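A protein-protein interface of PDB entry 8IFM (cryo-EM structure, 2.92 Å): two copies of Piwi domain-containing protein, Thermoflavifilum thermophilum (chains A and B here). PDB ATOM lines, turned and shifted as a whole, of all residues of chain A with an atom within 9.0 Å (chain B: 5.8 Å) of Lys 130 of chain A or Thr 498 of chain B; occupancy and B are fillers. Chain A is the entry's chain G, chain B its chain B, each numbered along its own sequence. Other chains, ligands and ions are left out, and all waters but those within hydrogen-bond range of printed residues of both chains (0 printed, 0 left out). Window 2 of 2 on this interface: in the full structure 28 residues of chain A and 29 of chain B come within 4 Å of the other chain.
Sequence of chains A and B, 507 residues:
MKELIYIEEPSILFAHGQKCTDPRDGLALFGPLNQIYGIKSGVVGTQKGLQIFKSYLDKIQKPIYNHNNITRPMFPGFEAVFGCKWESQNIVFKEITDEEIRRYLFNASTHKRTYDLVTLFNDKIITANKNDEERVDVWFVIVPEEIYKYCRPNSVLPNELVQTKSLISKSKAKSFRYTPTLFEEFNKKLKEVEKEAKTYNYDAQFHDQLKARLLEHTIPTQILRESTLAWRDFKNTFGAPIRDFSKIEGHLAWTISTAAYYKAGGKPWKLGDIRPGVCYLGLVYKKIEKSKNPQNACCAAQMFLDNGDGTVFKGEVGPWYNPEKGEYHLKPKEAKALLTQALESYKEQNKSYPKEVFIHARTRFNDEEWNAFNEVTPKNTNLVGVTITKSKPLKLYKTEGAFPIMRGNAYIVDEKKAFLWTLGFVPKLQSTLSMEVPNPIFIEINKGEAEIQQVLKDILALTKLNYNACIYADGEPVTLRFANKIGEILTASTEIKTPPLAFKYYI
The backbone carbonyl oxygen (O) of Lys 130 of chain A sits close to the backbone carbonyl oxygen (O) of Pro 500 of chain B (2.7 Å).
The side-chain hydroxyl (OH) of Tyr 505 of chain B lies within hydrogen-bond range of the backbone carbonyl oxygen (O) of Asn 129 of chain A, at 2.5 Å.
OG1 of Thr 218 of chain B sits close to ND2 of Asn 129 of chain A, 3.4 Å away.
The backbone carbonyl oxygen (O) of Pro 500 of chain B sits close to the side-chain amide oxygen (OD1) of Asn 131 of chain A.
CG of Lys 130 of chain A touches CG2 of Thr 218 of chain B, 3.6 Å away.
Lys 130 of chain A touches Thr 498 of chain B.
Ala 502 of chain B touches Lys 130 of chain A.
Lys 130 of chain A touches Tyr 505 of chain B (O to CE2, 3.3 Å).
Asn 131 of chain A touches Leu 501 of chain B.
CB of Ala 502 of chain B touches O of Asn 131 of chain A (3.2 Å).
Of chain B, only Thr 218, Thr 498, Pro 500, Ala 502 and Tyr 505 come within 4 Å of Lys 130 of chain A.
Thr 498 of chain B touches just one residue of chain A: Lys 130 (3.7 Å).
No residue of chain A comes within 4 Å of Pro 499 of chain B.
Pro 500 of chain B touches just these residues of chain A: Lys 130 (2.7 Å) and Asn 131 (2.8 Å).
Of the printed residues of chain A, Tyr 505 of chain B touches Asn 129 and Lys 130.
Printed residues of chain B within 4 Å of Asn 131 of chain A: Pro 500, Leu 501 and Ala 502.
Ile 125 of chain A touches none of the printed residues of chain B.
The nearest residue of chain B that does not touch Lys 130 of chain A is Leu 501 of chain B (4.1 Å).
The nearest residue of chain A that does not touch Thr 498 of chain B is Asn 131 of chain A (6.6 Å).
The nearest printed residue of chain A that does not touch Leu 501 of chain B is Lys 130 of chain A (4.1 Å).
Hydrophobic or aromatic side chains of chain B that line the printed part of chain A: Pro 500, Leu 501, Ala 502 and Tyr 505.
No position is printed for both chains.
Of the 10 pairs that touch across the chains among the printed residues, none has its exchanged pair printed and touching as well.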
ATOM      1  N   LYS A  94      -7.175 -11.086 -16.268  1.00  0.00           N
ATOM      2  CA  LYS A  94      -7.806 -10.798 -14.981  1.00  0.00           C
ATOM      3  C   LYS A  94      -6.718 -10.836 -13.914  1.00  0.00           C
ATOM      4  O   LYS A  94      -6.318 -11.913 -13.460  1.00  0.00           O
ATOM      5  CB  LYS A  94      -8.925 -11.786 -14.683  1.00  0.00           C
ATOM      6  CG  LYS A  94     -10.065 -11.704 -15.670  1.00  0.00           C
ATOM      7  CD  LYS A  94     -10.808 -10.394 -15.515  1.00  0.00           C
ATOM      8  CE  LYS A  94     -11.224  -9.840 -16.862  1.00  0.00           C
ATOM      9  NZ  LYS A  94     -11.063  -8.363 -16.921  1.00  0.00           N
ATOM     10  N   ASN A 122     -11.883 -18.322  -9.079  1.00  0.00           N
ATOM     11  CA  ASN A 122     -13.242 -18.655  -9.479  1.00  0.00           C
ATOM     12  C   ASN A 122     -14.051 -17.397  -9.749  1.00  0.00           C
ATOM     13  O   ASN A 122     -14.507 -17.174 -10.872  1.00  0.00           O
ATOM     14  CB  ASN A 122     -13.906 -19.502  -8.393  1.00  0.00           C
ATOM     15  CG  ASN A 122     -14.816 -20.568  -8.962  1.00  0.00           C
ATOM     16  OD1 ASN A 122     -14.372 -21.453  -9.690  1.00  0.00           O
ATOM     17  ND2 ASN A 122     -16.100 -20.485  -8.636  1.00  0.00           N
ATOM     18  N   ASP A 123     -14.206 -16.543  -8.734  1.00  0.00           N
ATOM     19  CA  ASP A 123     -15.048 -15.367  -8.896  1.00  0.00           C
ATOM     20  C   ASP A 123     -14.449 -14.387  -9.893  1.00  0.00           C
ATOM     21  O   ASP A 123     -15.199 -13.676 -10.566  1.00  0.00           O
ATOM     22  CB  ASP A 123     -15.324 -14.696  -7.541  1.00  0.00           C
ATOM     23  CG  ASP A 123     -14.075 -14.158  -6.859  1.00  0.00           C
ATOM     24  OD1 ASP A 123     -13.050 -13.931  -7.527  1.00  0.00           O
ATOM     25  OD2 ASP A 123     -14.124 -13.958  -5.627  1.00  0.00           O
ATOM     26  N   LYS A 124     -13.119 -14.352 -10.038  1.00  0.00           N
ATOM     27  CA  LYS A 124     -12.546 -13.594 -11.147  1.00  0.00           C
ATOM     28  C   LYS A 124     -13.096 -14.092 -12.479  1.00  0.00           C
ATOM     29  O   LYS A 124     -13.566 -13.302 -13.310  1.00  0.00           O
ATOM     30  CB  LYS A 124     -11.022 -13.693 -11.124  1.00  0.00           C
ATOM     31  CG  LYS A 124     -10.315 -12.377 -10.863  1.00  0.00           C
ATOM     32  CD  LYS A 124     -10.381 -11.991  -9.398  1.00  0.00           C
ATOM     33  CE  LYS A 124      -9.258 -11.035  -9.036  1.00  0.00           C
ATOM     34  NZ  LYS A 124      -9.532  -9.653  -9.514  1.00  0.00           N
ATOM     35  N   ILE A 125     -13.085 -15.412 -12.678  1.00  0.00           N
ATOM     36  CA  ILE A 125     -13.556 -15.983 -13.936  1.00  0.00           C
ATOM     37  C   ILE A 125     -15.048 -15.731 -14.124  1.00  0.00           C
ATOM     38  O   ILE A 125     -15.498 -15.412 -15.229  1.00  0.00           O
ATOM     39  CB  ILE A 125     -13.218 -17.485 -13.995  1.00  0.00           C
ATOM     40  CG1 ILE A 125     -11.710 -17.682 -14.157  1.00  0.00           C
ATOM     41  CG2 ILE A 125     -13.966 -18.164 -15.129  1.00  0.00           C
ATOM     42  CD1 ILE A 125     -11.258 -19.108 -13.959  1.00  0.00           C
ATOM     43  N   ILE A 126     -15.840 -15.876 -13.060  1.00  0.00           N
ATOM     44  CA  ILE A 126     -17.288 -15.714 -13.193  1.00  0.00           C
ATOM     45  C   ILE A 126     -17.654 -14.259 -13.459  1.00  0.00           C
ATOM     46  O   ILE A 126     -18.552 -13.977 -14.259  1.00  0.00           O
ATOM     47  CB  ILE A 126     -18.039 -16.265 -11.967  1.00  0.00           C
ATOM     48  CG1 ILE A 126     -17.340 -17.494 -11.395  1.00  0.00           C
ATOM     49  CG2 ILE A 126     -19.473 -16.606 -12.336  1.00  0.00           C
ATOM     50  CD1 ILE A 126     -17.729 -17.808  -9.969  1.00  0.00           C
ATOM     51  N   THR A 127     -16.992 -13.313 -12.791  1.00  0.00           N
ATOM     52  CA  THR A 127     -17.261 -11.907 -13.076  1.00  0.00           C
ATOM     53  C   THR A 127     -16.827 -11.537 -14.488  1.00  0.00           C
ATOM     54  O   THR A 127     -17.507 -10.759 -15.165  1.00  0.00           O
ATOM     55  CB  THR A 127     -16.574 -11.008 -12.048  1.00  0.00           C
ATOM     56  OG1 THR A 127     -15.163 -11.259 -12.051  1.00  0.00           O
ATOM     57  CG2 THR A 127     -17.143 -11.247 -10.657  1.00  0.00           C
ATOM     58  N   ALA A 128     -15.699 -12.081 -14.952  1.00  0.00           N
ATOM     59  CA  ALA A 128     -15.258 -11.787 -16.312  1.00  0.00           C
ATOM     60  C   ALA A 128     -16.198 -12.394 -17.348  1.00  0.00           C
ATOM     61  O   ALA A 128     -16.479 -11.773 -18.378  1.00  0.00           O
ATOM     62  CB  ALA A 128     -13.833 -12.287 -16.514  1.00  0.00           C
ATOM     63  N   ASN A 129     -16.693 -13.606 -17.096  1.00  0.00           N
ATOM     64  CA  ASN A 129     -17.619 -14.240 -18.027  1.00  0.00           C
ATOM     65  C   ASN A 129     -18.998 -13.600 -17.961  1.00  0.00           C
ATOM     66  O   ASN A 129     -19.751 -13.643 -18.940  1.00  0.00           O
ATOM     67  CB  ASN A 129     -17.702 -15.739 -17.731  1.00  0.00           C
ATOM     68  CG  ASN A 129     -18.873 -16.410 -18.421  1.00  0.00           C
ATOM     69  OD1 ASN A 129     -19.972 -16.482 -17.873  1.00  0.00           O
ATOM     70  ND2 ASN A 129     -18.642 -16.902 -19.631  1.00  0.00           N
ATOM     71  N   LYS A 130     -19.336 -12.997 -16.825  1.00  0.00           N
ATOM     72  CA  LYS A 130     -20.635 -12.370 -16.636  1.00  0.00           C
ATOM     73  C   LYS A 130     -20.614 -10.917 -17.098  1.00  0.00           C
ATOM     74  O   LYS A 130     -21.398 -10.525 -17.966  1.00  0.00           O
ATOM     75  CB  LYS A 130     -21.047 -12.463 -15.161  1.00  0.00           C
ATOM     76  CG  LYS A 130     -21.968 -13.630 -14.835  1.00  0.00           C
ATOM     77  CD  LYS A 130     -22.357 -13.677 -13.358  1.00  0.00           C
ATOM     78  CE  LYS A 130     -21.336 -12.983 -12.467  1.00  0.00           C
ATOM     79  NZ  LYS A 130     -21.747 -12.994 -11.035  1.00  0.00           N
ATOM     80  N   ASN A 131     -19.710 -10.114 -16.534  1.00  0.00           N
ATOM     81  CA  ASN A 131     -19.746  -8.669 -16.732  1.00  0.00           C
ATOM     82  C   ASN A 131     -19.027  -8.247 -18.008  1.00  0.00           C
ATOM     83  O   ASN A 131     -19.519  -7.390 -18.749  1.00  0.00           O
ATOM     84  CB  ASN A 131     -19.134  -7.966 -15.519  1.00  0.00           C
ATOM     85  CG  ASN A 131     -19.630  -8.534 -14.206  1.00  0.00           C
ATOM     86  OD1 ASN A 131     -20.583  -9.308 -14.172  1.00  0.00           O
ATOM     87  ND2 ASN A 131     -18.983  -8.147 -13.113  1.00  0.00           N
ATOM     88  N   ASP A 132     -17.857  -8.822 -18.275  1.00  0.00           N
ATOM     89  CA  ASP A 132     -17.032  -8.344 -19.377  1.00  0.00           C
ATOM     90  C   ASP A 132     -17.660  -8.671 -20.726  1.00  0.00           C
ATOM     91  O   ASP A 132     -18.260  -9.731 -20.916  1.00  0.00           O
ATOM     92  CB  ASP A 132     -15.629  -8.942 -19.297  1.00  0.00           C
ATOM     93  CG  ASP A 132     -14.845  -8.420 -18.113  1.00  0.00           C
ATOM     94  OD1 ASP A 132     -15.468  -8.093 -17.081  1.00  0.00           O
ATOM     95  OD2 ASP A 132     -13.606  -8.321 -18.221  1.00  0.00           O
ATOM     96  N   GLU A 133     -17.515  -7.734 -21.666  1.00  0.00           N
ATOM     97  CA  GLU A 133     -18.064  -7.896 -23.008  1.00  0.00           C
ATOM     98  C   GLU A 133     -17.211  -8.835 -23.856  1.00  0.00           C
ATOM     99  O   GLU A 133     -17.745  -9.611 -24.655  1.00  0.00           O
ATOM    100  CB  GLU A 133     -18.183  -6.520 -23.674  1.00  0.00           C
ATOM    101  CG  GLU A 133     -18.551  -6.480 -25.167  1.00  0.00           C
ATOM    102  CD  GLU A 133     -19.535  -7.551 -25.618  1.00  0.00           C
ATOM    103  OE1 GLU A 133     -19.453  -7.955 -26.794  1.00  0.00           O
ATOM    104  OE2 GLU A 133     -20.421  -7.951 -24.833  1.00  0.00           O
ATOM    105  N   GLU A 134     -15.892  -8.784 -23.691  1.00  0.00           N
ATOM    106  CA  GLU A 134     -15.000  -9.583 -24.521  1.00  0.00           C
ATOM    107  C   GLU A 134     -15.203 -11.070 -24.251  1.00  0.00           C
ATOM    108  O   GLU A 134     -15.209 -11.510 -23.097  1.00  0.00           O
ATOM    109  CB  GLU A 134     -13.547  -9.186 -24.263  1.00  0.00           C
ATOM    110  CG  GLU A 134     -13.164  -9.147 -22.792  1.00  0.00           C
ATOM    111  CD  GLU A 134     -13.251  -7.752 -22.205  1.00  0.00           C
ATOM    112  OE1 GLU A 134     -13.789  -6.853 -22.885  1.00  0.00           O
ATOM    113  OE2 GLU A 134     -12.788  -7.556 -21.061  1.00  0.00           O
ATOM    114  N   TRP A 139     -10.388 -20.401 -20.456  1.00  0.00           N
ATOM    115  CA  TRP A 139      -9.718 -19.580 -19.456  1.00  0.00           C
ATOM    116  C   TRP A 139      -8.475 -20.304 -18.960  1.00  0.00           C
ATOM    117  O   TRP A 139      -8.573 -21.403 -18.411  1.00  0.00           O
ATOM    118  CB  TRP A 139     -10.655 -19.270 -18.288  1.00  0.00           C
ATOM    119  CG  TRP A 139     -11.536 -18.100 -18.546  1.00  0.00           C
ATOM    120  CD1 TRP A 139     -12.786 -18.119 -19.089  1.00  0.00           C
ATOM    121  CD2 TRP A 139     -11.226 -16.726 -18.302  1.00  0.00           C
ATOM    122  NE1 TRP A 139     -13.280 -16.843 -19.186  1.00  0.00           N
ATOM    123  CE2 TRP A 139     -12.339 -15.969 -18.710  1.00  0.00           C
ATOM    124  CE3 TRP A 139     -10.116 -16.062 -17.773  1.00  0.00           C
ATOM    125  CZ2 TRP A 139     -12.374 -14.584 -18.607  1.00  0.00           C
ATOM    126  CZ3 TRP A 139     -10.154 -14.688 -17.671  1.00  0.00           C
ATOM    127  CH2 TRP A 139     -11.273 -13.964 -18.086  1.00  0.00           C
ATOM    128  N   HIS A 217     -21.902 -22.721 -13.930  1.00  0.00           N
ATOM    129  CA  HIS A 217     -21.784 -21.786 -15.046  1.00  0.00           C
ATOM    130  C   HIS A 217     -20.673 -22.315 -15.946  1.00  0.00           C
ATOM    131  O   HIS A 217     -19.493 -22.033 -15.739  1.00  0.00           O
ATOM    132  CB  HIS A 217     -21.506 -20.372 -14.547  1.00  0.00           C
ATOM    133  CG  HIS A 217     -20.654 -20.321 -13.316  1.00  0.00           C
ATOM    134  ND1 HIS A 217     -21.160 -19.990 -12.077  1.00  0.00           N
ATOM    135  CD2 HIS A 217     -19.334 -20.557 -13.132  1.00  0.00           C
ATOM    136  CE1 HIS A 217     -20.188 -20.025 -11.183  1.00  0.00           C
ATOM    137  NE2 HIS A 217     -19.069 -20.367 -11.798  1.00  0.00           N
ATOM    138  N   ILE A 219     -17.840 -23.104 -17.956  1.00  0.00           N
ATOM    139  CA  ILE A 219     -16.724 -22.326 -18.483  1.00  0.00           C
ATOM    140  C   ILE A 219     -15.544 -23.267 -18.691  1.00  0.00           C
ATOM    141  O   ILE A 219     -14.923 -23.703 -17.710  1.00  0.00           O
ATOM    142  CB  ILE A 219     -16.351 -21.173 -17.539  1.00  0.00           C
ATOM    143  CG1 ILE A 219     -17.478 -20.143 -17.473  1.00  0.00           C
ATOM    144  CG2 ILE A 219     -15.063 -20.508 -17.991  1.00  0.00           C
ATOM    145  CD1 ILE A 219     -17.311 -19.136 -16.363  1.00  0.00           C
ATOM    146  N   THR B 218     -24.538 -17.817 -18.377  1.00  0.00           N
ATOM    147  CA  THR B 218     -24.307 -16.789 -19.386  1.00  0.00           C
ATOM    148  C   THR B 218     -24.135 -17.375 -20.780  1.00  0.00           C
ATOM    149  O   THR B 218     -23.133 -18.037 -21.066  1.00  0.00           O
ATOM    150  CB  THR B 218     -23.074 -15.968 -19.019  1.00  0.00           C
ATOM    151  OG1 THR B 218     -21.963 -16.849 -18.811  1.00  0.00           O
ATOM    152  CG2 THR B 218     -23.324 -15.195 -17.748  1.00  0.00           C
ATOM    153  N   ILE B 496     -33.298 -13.385 -10.401  1.00  0.00           N
ATOM    154  CA  ILE B 496     -31.973 -13.953 -10.617  1.00  0.00           C
ATOM    155  C   ILE B 496     -30.987 -13.232  -9.709  1.00  0.00           C
ATOM    156  O   ILE B 496     -30.898 -11.999  -9.737  1.00  0.00           O
ATOM    157  CB  ILE B 496     -31.541 -13.840 -12.090  1.00  0.00           C
ATOM    158  CG1 ILE B 496     -32.583 -14.490 -13.005  1.00  0.00           C
ATOM    159  CG2 ILE B 496     -30.175 -14.473 -12.297  1.00  0.00           C
ATOM    160  CD1 ILE B 496     -33.358 -13.500 -13.851  1.00  0.00           C
ATOM    161  N   LYS B 497     -30.249 -13.997  -8.908  1.00  0.00           N
ATOM    162  CA  LYS B 497     -29.215 -13.431  -8.053  1.00  0.00           C
ATOM    163  C   LYS B 497     -27.948 -13.164  -8.853  1.00  0.00           C
ATOM    164  O   LYS B 497     -27.503 -14.010  -9.635  1.00  0.00           O
ATOM    165  CB  LYS B 497     -28.895 -14.368  -6.885  1.00  0.00           C
ATOM    166  CG  LYS B 497     -30.065 -14.763  -5.986  1.00  0.00           C
ATOM    167  CD  LYS B 497     -31.162 -13.710  -5.933  1.00  0.00           C
ATOM    168  CE  LYS B 497     -32.282 -14.142  -5.000  1.00  0.00           C
ATOM    169  NZ  LYS B 497     -33.290 -13.069  -4.784  1.00  0.00           N
ATOM    170  N   THR B 498     -27.361 -11.983  -8.635  1.00  0.00           N
ATOM    171  CA  THR B 498     -26.145 -11.528  -9.302  1.00  0.00           C
ATOM    172  C   THR B 498     -26.193 -11.819 -10.797  1.00  0.00           C
ATOM    173  O   THR B 498     -25.448 -12.677 -11.284  1.00  0.00           O
ATOM    174  CB  THR B 498     -24.909 -12.188  -8.683  1.00  0.00           C
ATOM    175  OG1 THR B 498     -24.889 -13.578  -9.023  1.00  0.00           O
ATOM    176  CG2 THR B 498     -24.930 -12.051  -7.167  1.00  0.00           C
ATOM    177  N   PRO B 499     -27.046 -11.138 -11.556  1.00  0.00           N
ATOM    178  CA  PRO B 499     -27.176 -11.445 -12.985  1.00  0.00           C
ATOM    179  C   PRO B 499     -25.917 -11.070 -13.750  1.00  0.00           C
ATOM    180  O   PRO B 499     -25.009 -10.436 -13.191  1.00  0.00           O
ATOM    181  CB  PRO B 499     -28.382 -10.591 -13.411  1.00  0.00           C
ATOM    182  CG  PRO B 499     -29.127 -10.318 -12.124  1.00  0.00           C
ATOM    183  CD  PRO B 499     -28.036 -10.138 -11.124  1.00  0.00           C
ATOM    184  N   PRO B 500     -25.821 -11.460 -15.029  1.00  0.00           N
ATOM    185  CA  PRO B 500     -24.543 -11.312 -15.749  1.00  0.00           C
ATOM    186  C   PRO B 500     -24.019  -9.889 -15.851  1.00  0.00           C
ATOM    187  O   PRO B 500     -22.798  -9.694 -15.838  1.00  0.00           O
ATOM    188  CB  PRO B 500     -24.866 -11.900 -17.124  1.00  0.00           C
ATOM    189  CG  PRO B 500     -25.887 -12.917 -16.850  1.00  0.00           C
ATOM    190  CD  PRO B 500     -26.747 -12.337 -15.762  1.00  0.00           C
ATOM    191  N   LEU B 501     -24.895  -8.887 -15.994  1.00  0.00           N
ATOM    192  CA  LEU B 501     -24.470  -7.486 -16.000  1.00  0.00           C
ATOM    193  C   LEU B 501     -23.665  -7.150 -17.263  1.00  0.00           C
ATOM    194  O   LEU B 501     -22.717  -6.368 -17.239  1.00  0.00           O
ATOM    195  CB  LEU B 501     -23.704  -7.197 -14.703  1.00  0.00           C
ATOM    196  CG  LEU B 501     -22.734  -6.085 -14.324  1.00  0.00           C
ATOM    197  CD1 LEU B 501     -23.470  -4.821 -14.129  1.00  0.00           C
ATOM    198  CD2 LEU B 501     -21.945  -6.453 -13.075  1.00  0.00           C
ATOM    199  N   ALA B 502     -24.065  -7.733 -18.393  1.00  0.00           N
ATOM    200  CA  ALA B 502     -23.430  -7.488 -19.684  1.00  0.00           C
ATOM    201  C   ALA B 502     -24.476  -7.620 -20.778  1.00  0.00           C
ATOM    202  O   ALA B 502     -25.278  -8.553 -20.761  1.00  0.00           O
ATOM    203  CB  ALA B 502     -22.277  -8.452 -19.954  1.00  0.00           C
ATOM    204  N   TYR B 505     -26.080 -10.570 -23.352  1.00  0.00           N
ATOM    205  CA  TYR B 505     -27.065 -11.525 -22.870  1.00  0.00           C
ATOM    206  C   TYR B 505     -28.482 -10.969 -22.858  1.00  0.00           C
ATOM    207  O   TYR B 505     -29.424 -11.730 -22.616  1.00  0.00           O
ATOM    208  CB  TYR B 505     -26.689 -11.990 -21.463  1.00  0.00           C
ATOM    209  CG  TYR B 505     -25.234 -12.366 -21.319  1.00  0.00           C
ATOM    210  CD1 TYR B 505     -24.699 -13.436 -22.018  1.00  0.00           C
ATOM    211  CD2 TYR B 505     -24.395 -11.646 -20.484  1.00  0.00           C
ATOM    212  CE1 TYR B 505     -23.371 -13.781 -21.884  1.00  0.00           C
ATOM    213  CE2 TYR B 505     -23.067 -11.986 -20.342  1.00  0.00           C
ATOM    214  CZ  TYR B 505     -22.560 -13.053 -21.046  1.00  0.00           C
ATOM    215  OH  TYR B 505     -21.235 -13.393 -20.911  1.00  0.00           O
